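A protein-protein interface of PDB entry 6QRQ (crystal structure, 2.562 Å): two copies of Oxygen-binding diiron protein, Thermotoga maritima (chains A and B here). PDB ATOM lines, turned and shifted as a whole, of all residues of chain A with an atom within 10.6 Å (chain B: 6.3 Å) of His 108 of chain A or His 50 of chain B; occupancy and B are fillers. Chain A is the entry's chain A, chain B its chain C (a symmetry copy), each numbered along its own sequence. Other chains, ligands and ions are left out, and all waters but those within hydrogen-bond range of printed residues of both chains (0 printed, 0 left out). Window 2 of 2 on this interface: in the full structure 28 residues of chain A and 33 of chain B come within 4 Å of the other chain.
The indole nitrogen of Trp 102 of chain A lies close to the side-chain amide nitrogen of Gln 76 of chain A (3.3 Å).
O of Asp 79 of chain B sits close to N of Gly 48 of chain B, 3.0 Å away.
Among the printed residues, pairs that only touch across the chains: Gln 76 of chain A with Pro 78 of chain B (3.3 Å), Phe 105 of chain A with Pro 78 of chain B (3.4 Å), Phe 105 of chain A with Asp 79 of chain B (3.3 Å), His 108 of chain A with Ile 27 of chain B (3.98 Å), His 108 of chain A with His 50 of chain B (3.7 Å), His 108 of chain A with Asp 79 of chain B (3.1 Å) and Phe 109 of chain A with Pro 78 of chain B (3.5 Å).
Of the printed residues of chain B, Phe 105 of chain A touches Pro 78 and Asp 79.
Of the printed residues of chain B, His 108 of chain A touches Ile 27 (3.98 Å), His 50 (3.7 Å) and Asp 79 (3.1 Å).
Of the printed residues of chain B, Phe 109 of chain A touches Pro 78.
Printed residues of chain A within 4 Å of Ile 27 of chain B: His 108.
No residue of chain A comes within 4 Å of Gly 48 of chain B.
No residue of chain A comes within 4 Å of Ala 49 of chain B.
Of chain A, only His 108 (3.7 Å) comes within 4 Å of His 50 of chain B.
Asp 79 of chain B touches just these residues of chain A: Phe 105 (3.3 Å) and His 108 (3.1 Å).
Of the 13 printed residues of chain B, 4 touch a printed residue of chain A.
Printed residues of chain B that touch a printed residue of chain A: Ile 27, His 50, Pro 78 and Asp 79.
Hydrophobic or aromatic side chains of chain B within 4 Å of the printed part of chain A: Ile 27, His 50 and Pro 78.
Of the 20 printed residues of chain A, 4 touch a printed residue of chain B.
Hydrophobic or aromatic side chains of chain A that line the printed part of chain B: Phe 105, His 108 and Phe 109.
Position printed for both chains: 82.
Of the 7 pairs that touch across the chains among the printed residues, none has its exchanged pair printed and touching as well.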
ATOM      1  N   GLN A  76       1.232  26.879  27.285  1.00  0.00           N
ATOM      2  CA  GLN A  76       0.372  26.587  26.154  1.00  0.00           C
ATOM      3  C   GLN A  76      -1.106  26.394  26.505  1.00  0.00           C
ATOM      4  O   GLN A  76      -1.498  26.093  27.630  1.00  0.00           O
ATOM      5  CB  GLN A  76       0.880  25.347  25.427  1.00  0.00           C
ATOM      6  CG  GLN A  76       0.343  24.067  26.024  1.00  0.00           C
ATOM      7  CD  GLN A  76       0.164  22.946  25.009  1.00  0.00           C
ATOM      8  OE1 GLN A  76       0.650  23.010  23.868  1.00  0.00           O
ATOM      9  NE2 GLN A  76      -0.536  21.905  25.424  1.00  0.00           N
ATOM     10  N   THR A  81      -3.154  29.093  21.979  1.00  0.00           N
ATOM     11  CA  THR A  81      -2.698  28.195  20.919  1.00  0.00           C
ATOM     12  C   THR A  81      -3.597  28.145  19.705  1.00  0.00           C
ATOM     13  O   THR A  81      -3.205  27.582  18.686  1.00  0.00           O
ATOM     14  CB  THR A  81      -2.398  26.788  21.433  1.00  0.00           C
ATOM     15  OG1 THR A  81      -3.581  25.968  21.472  1.00  0.00           O
ATOM     16  CG2 THR A  81      -1.446  26.699  22.547  1.00  0.00           C
ATOM     17  N   SER A  82      -4.779  28.710  19.768  1.00  0.00           N
ATOM     18  CA  SER A  82      -5.505  28.916  18.528  1.00  0.00           C
ATOM     19  C   SER A  82      -4.737  29.844  17.572  1.00  0.00           C
ATOM     20  O   SER A  82      -4.880  29.725  16.348  1.00  0.00           O
ATOM     21  CB  SER A  82      -6.898  29.487  18.852  1.00  0.00           C
ATOM     22  OG  SER A  82      -7.453  28.927  20.055  1.00  0.00           O
ATOM     23  N   GLY A  83      -3.924  30.773  18.105  1.00  0.00           N
ATOM     24  CA  GLY A  83      -3.278  31.829  17.341  1.00  0.00           C
ATOM     25  C   GLY A  83      -1.840  31.684  16.851  1.00  0.00           C
ATOM     26  O   GLY A  83      -1.368  32.562  16.122  1.00  0.00           O
ATOM     27  N   ILE A  84      -1.118  30.625  17.211  1.00  0.00           N
ATOM     28  CA  ILE A  84       0.310  30.586  16.889  1.00  0.00           C
ATOM     29  C   ILE A  84       0.553  30.701  15.385  1.00  0.00           C
ATOM     30  O   ILE A  84       1.465  31.415  14.948  1.00  0.00           O
ATOM     31  CB  ILE A  84       0.960  29.325  17.484  1.00  0.00           C
ATOM     32  CG1 ILE A  84       0.701  29.258  18.994  1.00  0.00           C
ATOM     33  CG2 ILE A  84       2.429  29.314  17.228  1.00  0.00           C
ATOM     34  CD1 ILE A  84       1.778  28.490  19.762  1.00  0.00           C
ATOM     35  N   LEU A  85      -0.217  29.984  14.562  1.00  0.00           N
ATOM     36  CA  LEU A  85       0.021  30.074  13.124  1.00  0.00           C
ATOM     37  C   LEU A  85      -0.363  31.444  12.570  1.00  0.00           C
ATOM     38  O   LEU A  85       0.261  31.925  11.619  1.00  0.00           O
ATOM     39  CB  LEU A  85      -0.712  28.956  12.387  1.00  0.00           C
ATOM     40  CG  LEU A  85      -0.377  28.771  10.901  1.00  0.00           C
ATOM     41  CD1 LEU A  85       1.095  28.449  10.621  1.00  0.00           C
ATOM     42  CD2 LEU A  85      -1.257  27.664  10.351  1.00  0.00           C
ATOM     43  N   LEU A 101       8.502  21.512  26.213  1.00  0.00           N
ATOM     44  CA  LEU A 101       7.580  20.420  26.504  1.00  0.00           C
ATOM     45  C   LEU A 101       6.476  20.323  25.476  1.00  0.00           C
ATOM     46  O   LEU A 101       5.966  19.231  25.230  1.00  0.00           O
ATOM     47  CB  LEU A 101       6.968  20.559  27.896  1.00  0.00           C
ATOM     48  CG  LEU A 101       7.763  19.824  28.977  1.00  0.00           C
ATOM     49  CD1 LEU A 101       9.276  20.128  28.877  1.00  0.00           C
ATOM     50  CD2 LEU A 101       7.244  20.206  30.323  1.00  0.00           C
ATOM     51  N   TRP A 102       6.104  21.432  24.852  1.00  0.00           N
ATOM     52  CA  TRP A 102       4.914  21.453  24.020  1.00  0.00           C
ATOM     53  C   TRP A 102       5.200  21.503  22.519  1.00  0.00           C
ATOM     54  O   TRP A 102       4.285  21.256  21.733  1.00  0.00           O
ATOM     55  CB  TRP A 102       4.014  22.629  24.455  1.00  0.00           C
ATOM     56  CG  TRP A 102       3.282  22.259  25.745  1.00  0.00           C
ATOM     57  CD1 TRP A 102       2.563  21.098  25.976  1.00  0.00           C
ATOM     58  CD2 TRP A 102       3.235  23.002  26.984  1.00  0.00           C
ATOM     59  NE1 TRP A 102       2.059  21.096  27.265  1.00  0.00           N
ATOM     60  CE2 TRP A 102       2.451  22.247  27.902  1.00  0.00           C
ATOM     61  CE3 TRP A 102       3.749  24.235  27.394  1.00  0.00           C
ATOM     62  CZ2 TRP A 102       2.187  22.687  29.197  1.00  0.00           C
ATOM     63  CZ3 TRP A 102       3.478  24.664  28.658  1.00  0.00           C
ATOM     64  CH2 TRP A 102       2.701  23.892  29.555  1.00  0.00           C
ATOM     65  N   VAL A 103       6.447  21.717  22.094  1.00  0.00           N
ATOM     66  CA  VAL A 103       6.716  21.995  20.683  1.00  0.00           C
ATOM     67  C   VAL A 103       6.371  20.849  19.740  1.00  0.00           C
ATOM     68  O   VAL A 103       6.427  21.029  18.523  1.00  0.00           O
ATOM     69  CB  VAL A 103       8.187  22.408  20.448  1.00  0.00           C
ATOM     70  CG1 VAL A 103       8.436  23.780  21.028  1.00  0.00           C
ATOM     71  CG2 VAL A 103       9.142  21.372  21.006  1.00  0.00           C
ATOM     72  N   ARG A 104       6.077  19.655  20.239  1.00  0.00           N
ATOM     73  CA  ARG A 104       5.689  18.590  19.318  1.00  0.00           C
ATOM     74  C   ARG A 104       4.193  18.294  19.358  1.00  0.00           C
ATOM     75  O   ARG A 104       3.746  17.255  18.874  1.00  0.00           O
ATOM     76  CB  ARG A 104       6.547  17.351  19.536  1.00  0.00           C
ATOM     77  CG  ARG A 104       8.009  17.740  19.263  1.00  0.00           C
ATOM     78  CD  ARG A 104       9.022  16.710  19.707  1.00  0.00           C
ATOM     79  NE  ARG A 104      10.351  16.901  19.118  1.00  0.00           N
ATOM     80  CZ  ARG A 104      10.637  17.017  17.818  1.00  0.00           C
ATOM     81  NH1 ARG A 104       9.694  16.969  16.878  1.00  0.00           N
ATOM     82  NH2 ARG A 104      11.907  17.172  17.454  1.00  0.00           N
ATOM     83  N   PHE A 105       3.421  19.182  19.950  1.00  0.00           N
ATOM     84  CA  PHE A 105       2.035  19.352  19.570  1.00  0.00           C
ATOM     85  C   PHE A 105       1.901  20.315  18.402  1.00  0.00           C
ATOM     86  O   PHE A 105       0.775  20.609  17.981  1.00  0.00           O
ATOM     87  CB  PHE A 105       1.222  19.908  20.752  1.00  0.00           C
ATOM     88  CG  PHE A 105       1.090  18.962  21.935  1.00  0.00           C
ATOM     89  CD1 PHE A 105       0.409  17.751  21.820  1.00  0.00           C
ATOM     90  CD2 PHE A 105       1.602  19.318  23.183  1.00  0.00           C
ATOM     91  CE1 PHE A 105       0.275  16.901  22.920  1.00  0.00           C
ATOM     92  CE2 PHE A 105       1.467  18.470  24.282  1.00  0.00           C
ATOM     93  CZ  PHE A 105       0.802  17.263  24.152  1.00  0.00           C
ATOM     94  N   LEU A 106       3.019  20.847  17.898  1.00  0.00           N
ATOM     95  CA  LEU A 106       2.942  21.921  16.915  1.00  0.00           C
ATOM     96  C   LEU A 106       2.369  21.471  15.572  1.00  0.00           C
ATOM     97  O   LEU A 106       1.599  22.234  14.975  1.00  0.00           O
ATOM     98  CB  LEU A 106       4.312  22.582  16.731  1.00  0.00           C
ATOM     99  CG  LEU A 106       4.674  23.617  17.805  1.00  0.00           C
ATOM    100  CD1 LEU A 106       5.924  24.392  17.430  1.00  0.00           C
ATOM    101  CD2 LEU A 106       3.538  24.563  18.075  1.00  0.00           C
ATOM    102  N   PRO A 107       2.716  20.283  15.042  1.00  0.00           N
ATOM    103  CA  PRO A 107       2.012  19.808  13.834  1.00  0.00           C
ATOM    104  C   PRO A 107       0.494  19.847  13.963  1.00  0.00           C
ATOM    105  O   PRO A 107      -0.196  20.293  13.035  1.00  0.00           O
ATOM    106  CB  PRO A 107       2.532  18.378  13.664  1.00  0.00           C
ATOM    107  CG  PRO A 107       3.874  18.383  14.315  1.00  0.00           C
ATOM    108  CD  PRO A 107       3.849  19.402  15.400  1.00  0.00           C
ATOM    109  N   HIS A 108      -0.047  19.423  15.106  1.00  0.00           N
ATOM    110  CA  HIS A 108      -1.494  19.403  15.318  1.00  0.00           C
ATOM    111  C   HIS A 108      -2.097  20.804  15.299  1.00  0.00           C
ATOM    112  O   HIS A 108      -3.314  20.977  15.420  1.00  0.00           O
ATOM    113  CB  HIS A 108      -1.823  18.671  16.620  1.00  0.00           C
ATOM    114  CG  HIS A 108      -1.232  17.299  16.684  1.00  0.00           C
ATOM    115  ND1 HIS A 108      -1.090  16.597  17.862  1.00  0.00           N
ATOM    116  CD2 HIS A 108      -0.720  16.508  15.710  1.00  0.00           C
ATOM    117  CE1 HIS A 108      -0.522  15.430  17.610  1.00  0.00           C
ATOM    118  NE2 HIS A 108      -0.287  15.352  16.312  1.00  0.00           N
ATOM    119  N   PHE A 109      -1.267  21.820  15.110  1.00  0.00           N
ATOM    120  CA  PHE A 109      -1.773  23.177  14.971  1.00  0.00           C
ATOM    121  C   PHE A 109      -1.335  23.786  13.649  1.00  0.00           C
ATOM    122  O   PHE A 109      -1.341  25.013  13.495  1.00  0.00           O
ATOM    123  CB  PHE A 109      -1.340  24.041  16.153  1.00  0.00           C
ATOM    124  CG  PHE A 109      -2.050  23.699  17.418  1.00  0.00           C
ATOM    125  CD1 PHE A 109      -1.613  22.646  18.202  1.00  0.00           C
ATOM    126  CD2 PHE A 109      -3.182  24.412  17.818  1.00  0.00           C
ATOM    127  CE1 PHE A 109      -2.284  22.315  19.377  1.00  0.00           C
ATOM    128  CE2 PHE A 109      -3.856  24.083  18.988  1.00  0.00           C
ATOM    129  CZ  PHE A 109      -3.409  23.038  19.767  1.00  0.00           C
ATOM    130  N   GLY A 110      -0.956  22.943  12.691  1.00  0.00           N
ATOM    131  CA  GLY A 110      -0.564  23.419  11.391  1.00  0.00           C
ATOM    132  C   GLY A 110       0.810  24.022  11.336  1.00  0.00           C
ATOM    133  O   GLY A 110       1.189  24.555  10.288  1.00  0.00           O
ATOM    134  N   ILE A 111       1.573  23.949  12.421  1.00  0.00           N
ATOM    135  CA  ILE A 111       2.929  24.474  12.452  1.00  0.00           C
ATOM    136  C   ILE A 111       3.822  23.296  12.100  1.00  0.00           C
ATOM    137  O   ILE A 111       4.038  22.400  12.910  1.00  0.00           O
ATOM    138  CB  ILE A 111       3.301  25.095  13.803  1.00  0.00           C
ATOM    139  CG1 ILE A 111       2.625  26.457  14.008  1.00  0.00           C
ATOM    140  CG2 ILE A 111       4.830  25.312  13.891  1.00  0.00           C
ATOM    141  CD1 ILE A 111       1.205  26.407  14.488  1.00  0.00           C
ATOM    142  N   TYR A 112       4.309  23.280  10.862  1.00  0.00           N
ATOM    143  CA  TYR A 112       5.194  22.229  10.381  1.00  0.00           C
ATOM    144  C   TYR A 112       6.614  22.709  10.196  1.00  0.00           C
ATOM    145  O   TYR A 112       7.537  21.887  10.195  1.00  0.00           O
ATOM    146  CB  TYR A 112       4.683  21.651   9.055  1.00  0.00           C
ATOM    147  CG  TYR A 112       3.452  20.779   9.222  1.00  0.00           C
ATOM    148  CD1 TYR A 112       3.567  19.423   9.523  1.00  0.00           C
ATOM    149  CD2 TYR A 112       2.172  21.317   9.097  1.00  0.00           C
ATOM    150  CE1 TYR A 112       2.454  18.628   9.682  1.00  0.00           C
ATOM    151  CE2 TYR A 112       1.051  20.530   9.259  1.00  0.00           C
ATOM    152  CZ  TYR A 112       1.198  19.187   9.552  1.00  0.00           C
ATOM    153  OH  TYR A 112       0.082  18.400   9.714  1.00  0.00           O
ATOM    154  N   ASP A 113       6.814  24.009  10.045  1.00  0.00           N
ATOM    155  CA  ASP A 113       8.141  24.580   9.917  1.00  0.00           C
ATOM    156  C   ASP A 113       8.495  25.230  11.248  1.00  0.00           C
ATOM    157  O   ASP A 113       7.858  26.208  11.664  1.00  0.00           O
ATOM    158  CB  ASP A 113       8.179  25.596   8.780  1.00  0.00           C
ATOM    159  CG  ASP A 113       9.579  26.112   8.513  1.00  0.00           C
ATOM    160  OD1 ASP A 113      10.500  25.661   9.225  1.00  0.00           O
ATOM    161  OD2 ASP A 113       9.763  26.957   7.605  1.00  0.00           O
ATOM    162  N   GLN A 114       9.516  24.690  11.915  1.00  0.00           N
ATOM    163  CA  GLN A 114       9.929  25.198  13.217  1.00  0.00           C
ATOM    164  C   GLN A 114      11.215  26.020  13.155  1.00  0.00           C
ATOM    165  O   GLN A 114      11.894  26.177  14.175  1.00  0.00           O
ATOM    166  CB  GLN A 114      10.079  24.046  14.206  1.00  0.00           C
ATOM    167  CG  GLN A 114       8.768  23.458  14.690  1.00  0.00           C
ATOM    168  CD  GLN A 114       8.979  22.436  15.781  1.00  0.00           C
ATOM    169  OE1 GLN A 114       9.976  22.504  16.509  1.00  0.00           O
ATOM    170  NE2 GLN A 114       8.028  21.506  15.937  1.00  0.00           N
ATOM    171  N   ILE B  27       4.665  10.891  15.331  1.00  0.00           N
ATOM    172  CA  ILE B  27       3.678  10.905  16.405  1.00  0.00           C
ATOM    173  C   ILE B  27       3.993   9.781  17.385  1.00  0.00           C
ATOM    174  O   ILE B  27       4.486   8.724  16.982  1.00  0.00           O
ATOM    175  CB  ILE B  27       2.233  10.789  15.848  1.00  0.00           C
ATOM    176  CG1 ILE B  27       2.123   9.651  14.817  1.00  0.00           C
ATOM    177  CG2 ILE B  27       1.781  12.116  15.250  1.00  0.00           C
ATOM    178  CD1 ILE B  27       1.589   8.328  15.362  1.00  0.00           C
ATOM    179  N   THR B  30      -0.534   6.211  20.423  1.00  0.00           N
ATOM    180  CA  THR B  30      -1.639   6.527  21.298  1.00  0.00           C
ATOM    181  C   THR B  30      -2.590   5.344  21.302  1.00  0.00           C
ATOM    182  O   THR B  30      -2.799   4.702  20.266  1.00  0.00           O
ATOM    183  CB  THR B  30      -2.334   7.812  20.857  1.00  0.00           C
ATOM    184  OG1 THR B  30      -1.394   8.896  20.931  1.00  0.00           O
ATOM    185  CG2 THR B  30      -3.514   8.135  21.766  1.00  0.00           C
ATOM    186  N   GLY B  47      -9.418  10.074  19.988  1.00  0.00           N
ATOM    187  CA  GLY B  47      -8.409  10.847  19.284  1.00  0.00           C
ATOM    188  C   GLY B  47      -8.964  12.126  18.683  1.00  0.00           C
ATOM    189  O   GLY B  47     -10.115  12.182  18.214  1.00  0.00           O
ATOM    190  N   GLY B  48      -8.101  13.154  18.661  1.00  0.00           N
ATOM    191  CA  GLY B  48      -8.441  14.468  18.154  1.00  0.00           C
ATOM    192  C   GLY B  48      -8.485  14.497  16.643  1.00  0.00           C
ATOM    193  O   GLY B  48      -8.518  13.462  15.973  1.00  0.00           O
ATOM    194  N   ALA B  49      -8.479  15.716  16.096  1.00  0.00           N
ATOM    195  CA  ALA B  49      -8.835  15.889  14.692  1.00  0.00           C
ATOM    196  C   ALA B  49      -7.811  15.256  13.761  1.00  0.00           C
ATOM    197  O   ALA B  49      -8.174  14.802  12.673  1.00  0.00           O
ATOM    198  CB  ALA B  49      -8.998  17.369  14.370  1.00  0.00           C
ATOM    199  N   HIS B  50      -6.547  15.161  14.184  1.00  0.00           N
ATOM    200  CA  HIS B  50      -5.512  14.659  13.284  1.00  0.00           C
ATOM    201  C   HIS B  50      -5.736  13.192  12.965  1.00  0.00           C
ATOM    202  O   HIS B  50      -5.657  12.773  11.809  1.00  0.00           O
ATOM    203  CB  HIS B  50      -4.138  14.849  13.925  1.00  0.00           C
ATOM    204  CG  HIS B  50      -4.021  14.238  15.293  1.00  0.00           C
ATOM    205  ND1 HIS B  50      -4.777  14.661  16.369  1.00  0.00           N
ATOM    206  CD2 HIS B  50      -3.230  13.239  15.761  1.00  0.00           C
ATOM    207  CE1 HIS B  50      -4.462  13.948  17.437  1.00  0.00           C
ATOM    208  NE2 HIS B  50      -3.525  13.080  17.096  1.00  0.00           N
ATOM    209  N   VAL B  51      -6.080  12.408  13.978  1.00  0.00           N
ATOM    210  CA  VAL B  51      -6.297  10.984  13.828  1.00  0.00           C
ATOM    211  C   VAL B  51      -7.761  10.644  13.605  1.00  0.00           C
ATOM    212  O   VAL B  51      -8.099   9.464  13.443  1.00  0.00           O
ATOM    213  CB  VAL B  51      -5.722  10.274  15.068  1.00  0.00           C
ATOM    214  CG1 VAL B  51      -6.709  10.318  16.227  1.00  0.00           C
ATOM    215  CG2 VAL B  51      -5.259   8.886  14.723  1.00  0.00           C
ATOM    216  N   PHE B  52      -8.634  11.650  13.548  1.00  0.00           N
ATOM    217  CA  PHE B  52     -10.067  11.398  13.663  1.00  0.00           C
ATOM    218  C   PHE B  52     -10.644  10.465  12.607  1.00  0.00           C
ATOM    219  O   PHE B  52     -11.483   9.624  12.979  1.00  0.00           O
ATOM    220  CB  PHE B  52     -10.847  12.710  13.658  1.00  0.00           C
ATOM    221  CG  PHE B  52     -12.308  12.515  13.819  1.00  0.00           C
ATOM    222  CD1 PHE B  52     -12.854  12.314  15.075  1.00  0.00           C
ATOM    223  CD2 PHE B  52     -13.144  12.499  12.719  1.00  0.00           C
ATOM    224  CE1 PHE B  52     -14.217  12.116  15.228  1.00  0.00           C
ATOM    225  CE2 PHE B  52     -14.523  12.300  12.873  1.00  0.00           C
ATOM    226  CZ  PHE B  52     -15.050  12.107  14.120  1.00  0.00           C
ATOM    227  N   PRO B  53     -10.326  10.582  11.306  1.00  0.00           N
ATOM    228  CA  PRO B  53     -10.928   9.627  10.356  1.00  0.00           C
ATOM    229  C   PRO B  53     -10.747   8.178  10.776  1.00  0.00           C
ATOM    230  O   PRO B  53     -11.734   7.437  10.799  1.00  0.00           O
ATOM    231  CB  PRO B  53     -10.226   9.952   9.025  1.00  0.00           C
ATOM    232  CG  PRO B  53      -9.185  11.029   9.340  1.00  0.00           C
ATOM    233  CD  PRO B  53      -9.636  11.679  10.602  1.00  0.00           C
ATOM    234  N   PRO B  78      -3.950  18.984  23.811  1.00  0.00           N
ATOM    235  CA  PRO B  78      -4.295  19.724  22.582  1.00  0.00           C
ATOM    236  C   PRO B  78      -4.619  18.823  21.398  1.00  0.00           C
ATOM    237  O   PRO B  78      -5.334  19.258  20.484  1.00  0.00           O
ATOM    238  CB  PRO B  78      -3.050  20.591  22.324  1.00  0.00           C
ATOM    239  CG  PRO B  78      -1.966  20.001  23.144  1.00  0.00           C
ATOM    240  CD  PRO B  78      -2.628  19.358  24.332  1.00  0.00           C
ATOM    241  N   ASP B  79      -4.061  17.614  21.346  1.00  0.00           N
ATOM    242  CA  ASP B  79      -4.408  16.651  20.304  1.00  0.00           C
ATOM    243  C   ASP B  79      -5.677  15.830  20.590  1.00  0.00           C
ATOM    244  O   ASP B  79      -5.990  14.944  19.792  1.00  0.00           O
ATOM    245  CB  ASP B  79      -3.224  15.731  19.985  1.00  0.00           C
ATOM    246  CG  ASP B  79      -2.586  15.149  21.202  1.00  0.00           C
ATOM    247  OD1 ASP B  79      -3.233  15.133  22.266  1.00  0.00           O
ATOM    248  OD2 ASP B  79      -1.427  14.700  21.083  1.00  0.00           O
ATOM    249  N   VAL B  80      -6.331  15.975  21.749  1.00  0.00           N
ATOM    250  CA  VAL B  80      -7.684  15.429  21.899  1.00  0.00           C
ATOM    251  C   VAL B  80      -8.696  16.568  21.791  1.00  0.00           C
ATOM    252  O   VAL B  80      -9.849  16.362  21.398  1.00  0.00           O
ATOM    253  CB  VAL B  80      -7.912  14.665  23.229  1.00  0.00           C
ATOM    254  CG1 VAL B  80      -7.063  13.404  23.316  1.00  0.00           C
ATOM    255  CG2 VAL B  80      -7.759  15.584  24.457  1.00  0.00           C
ATOM    256  N   SER B  82      -8.979  19.005  19.735  1.00  0.00           N
ATOM    257  CA  SER B  82      -9.439  19.241  18.369  1.00  0.00           C
ATOM    258  C   SER B  82     -10.643  18.382  18.002  1.00  0.00           C
ATOM    259  O   SER B  82     -11.388  18.729  17.077  1.00  0.00           O
ATOM    260  CB  SER B  82      -8.306  19.009  17.389  1.00  0.00           C
ATOM    261  OG  SER B  82      -7.631  17.830  17.740  1.00  0.00           O
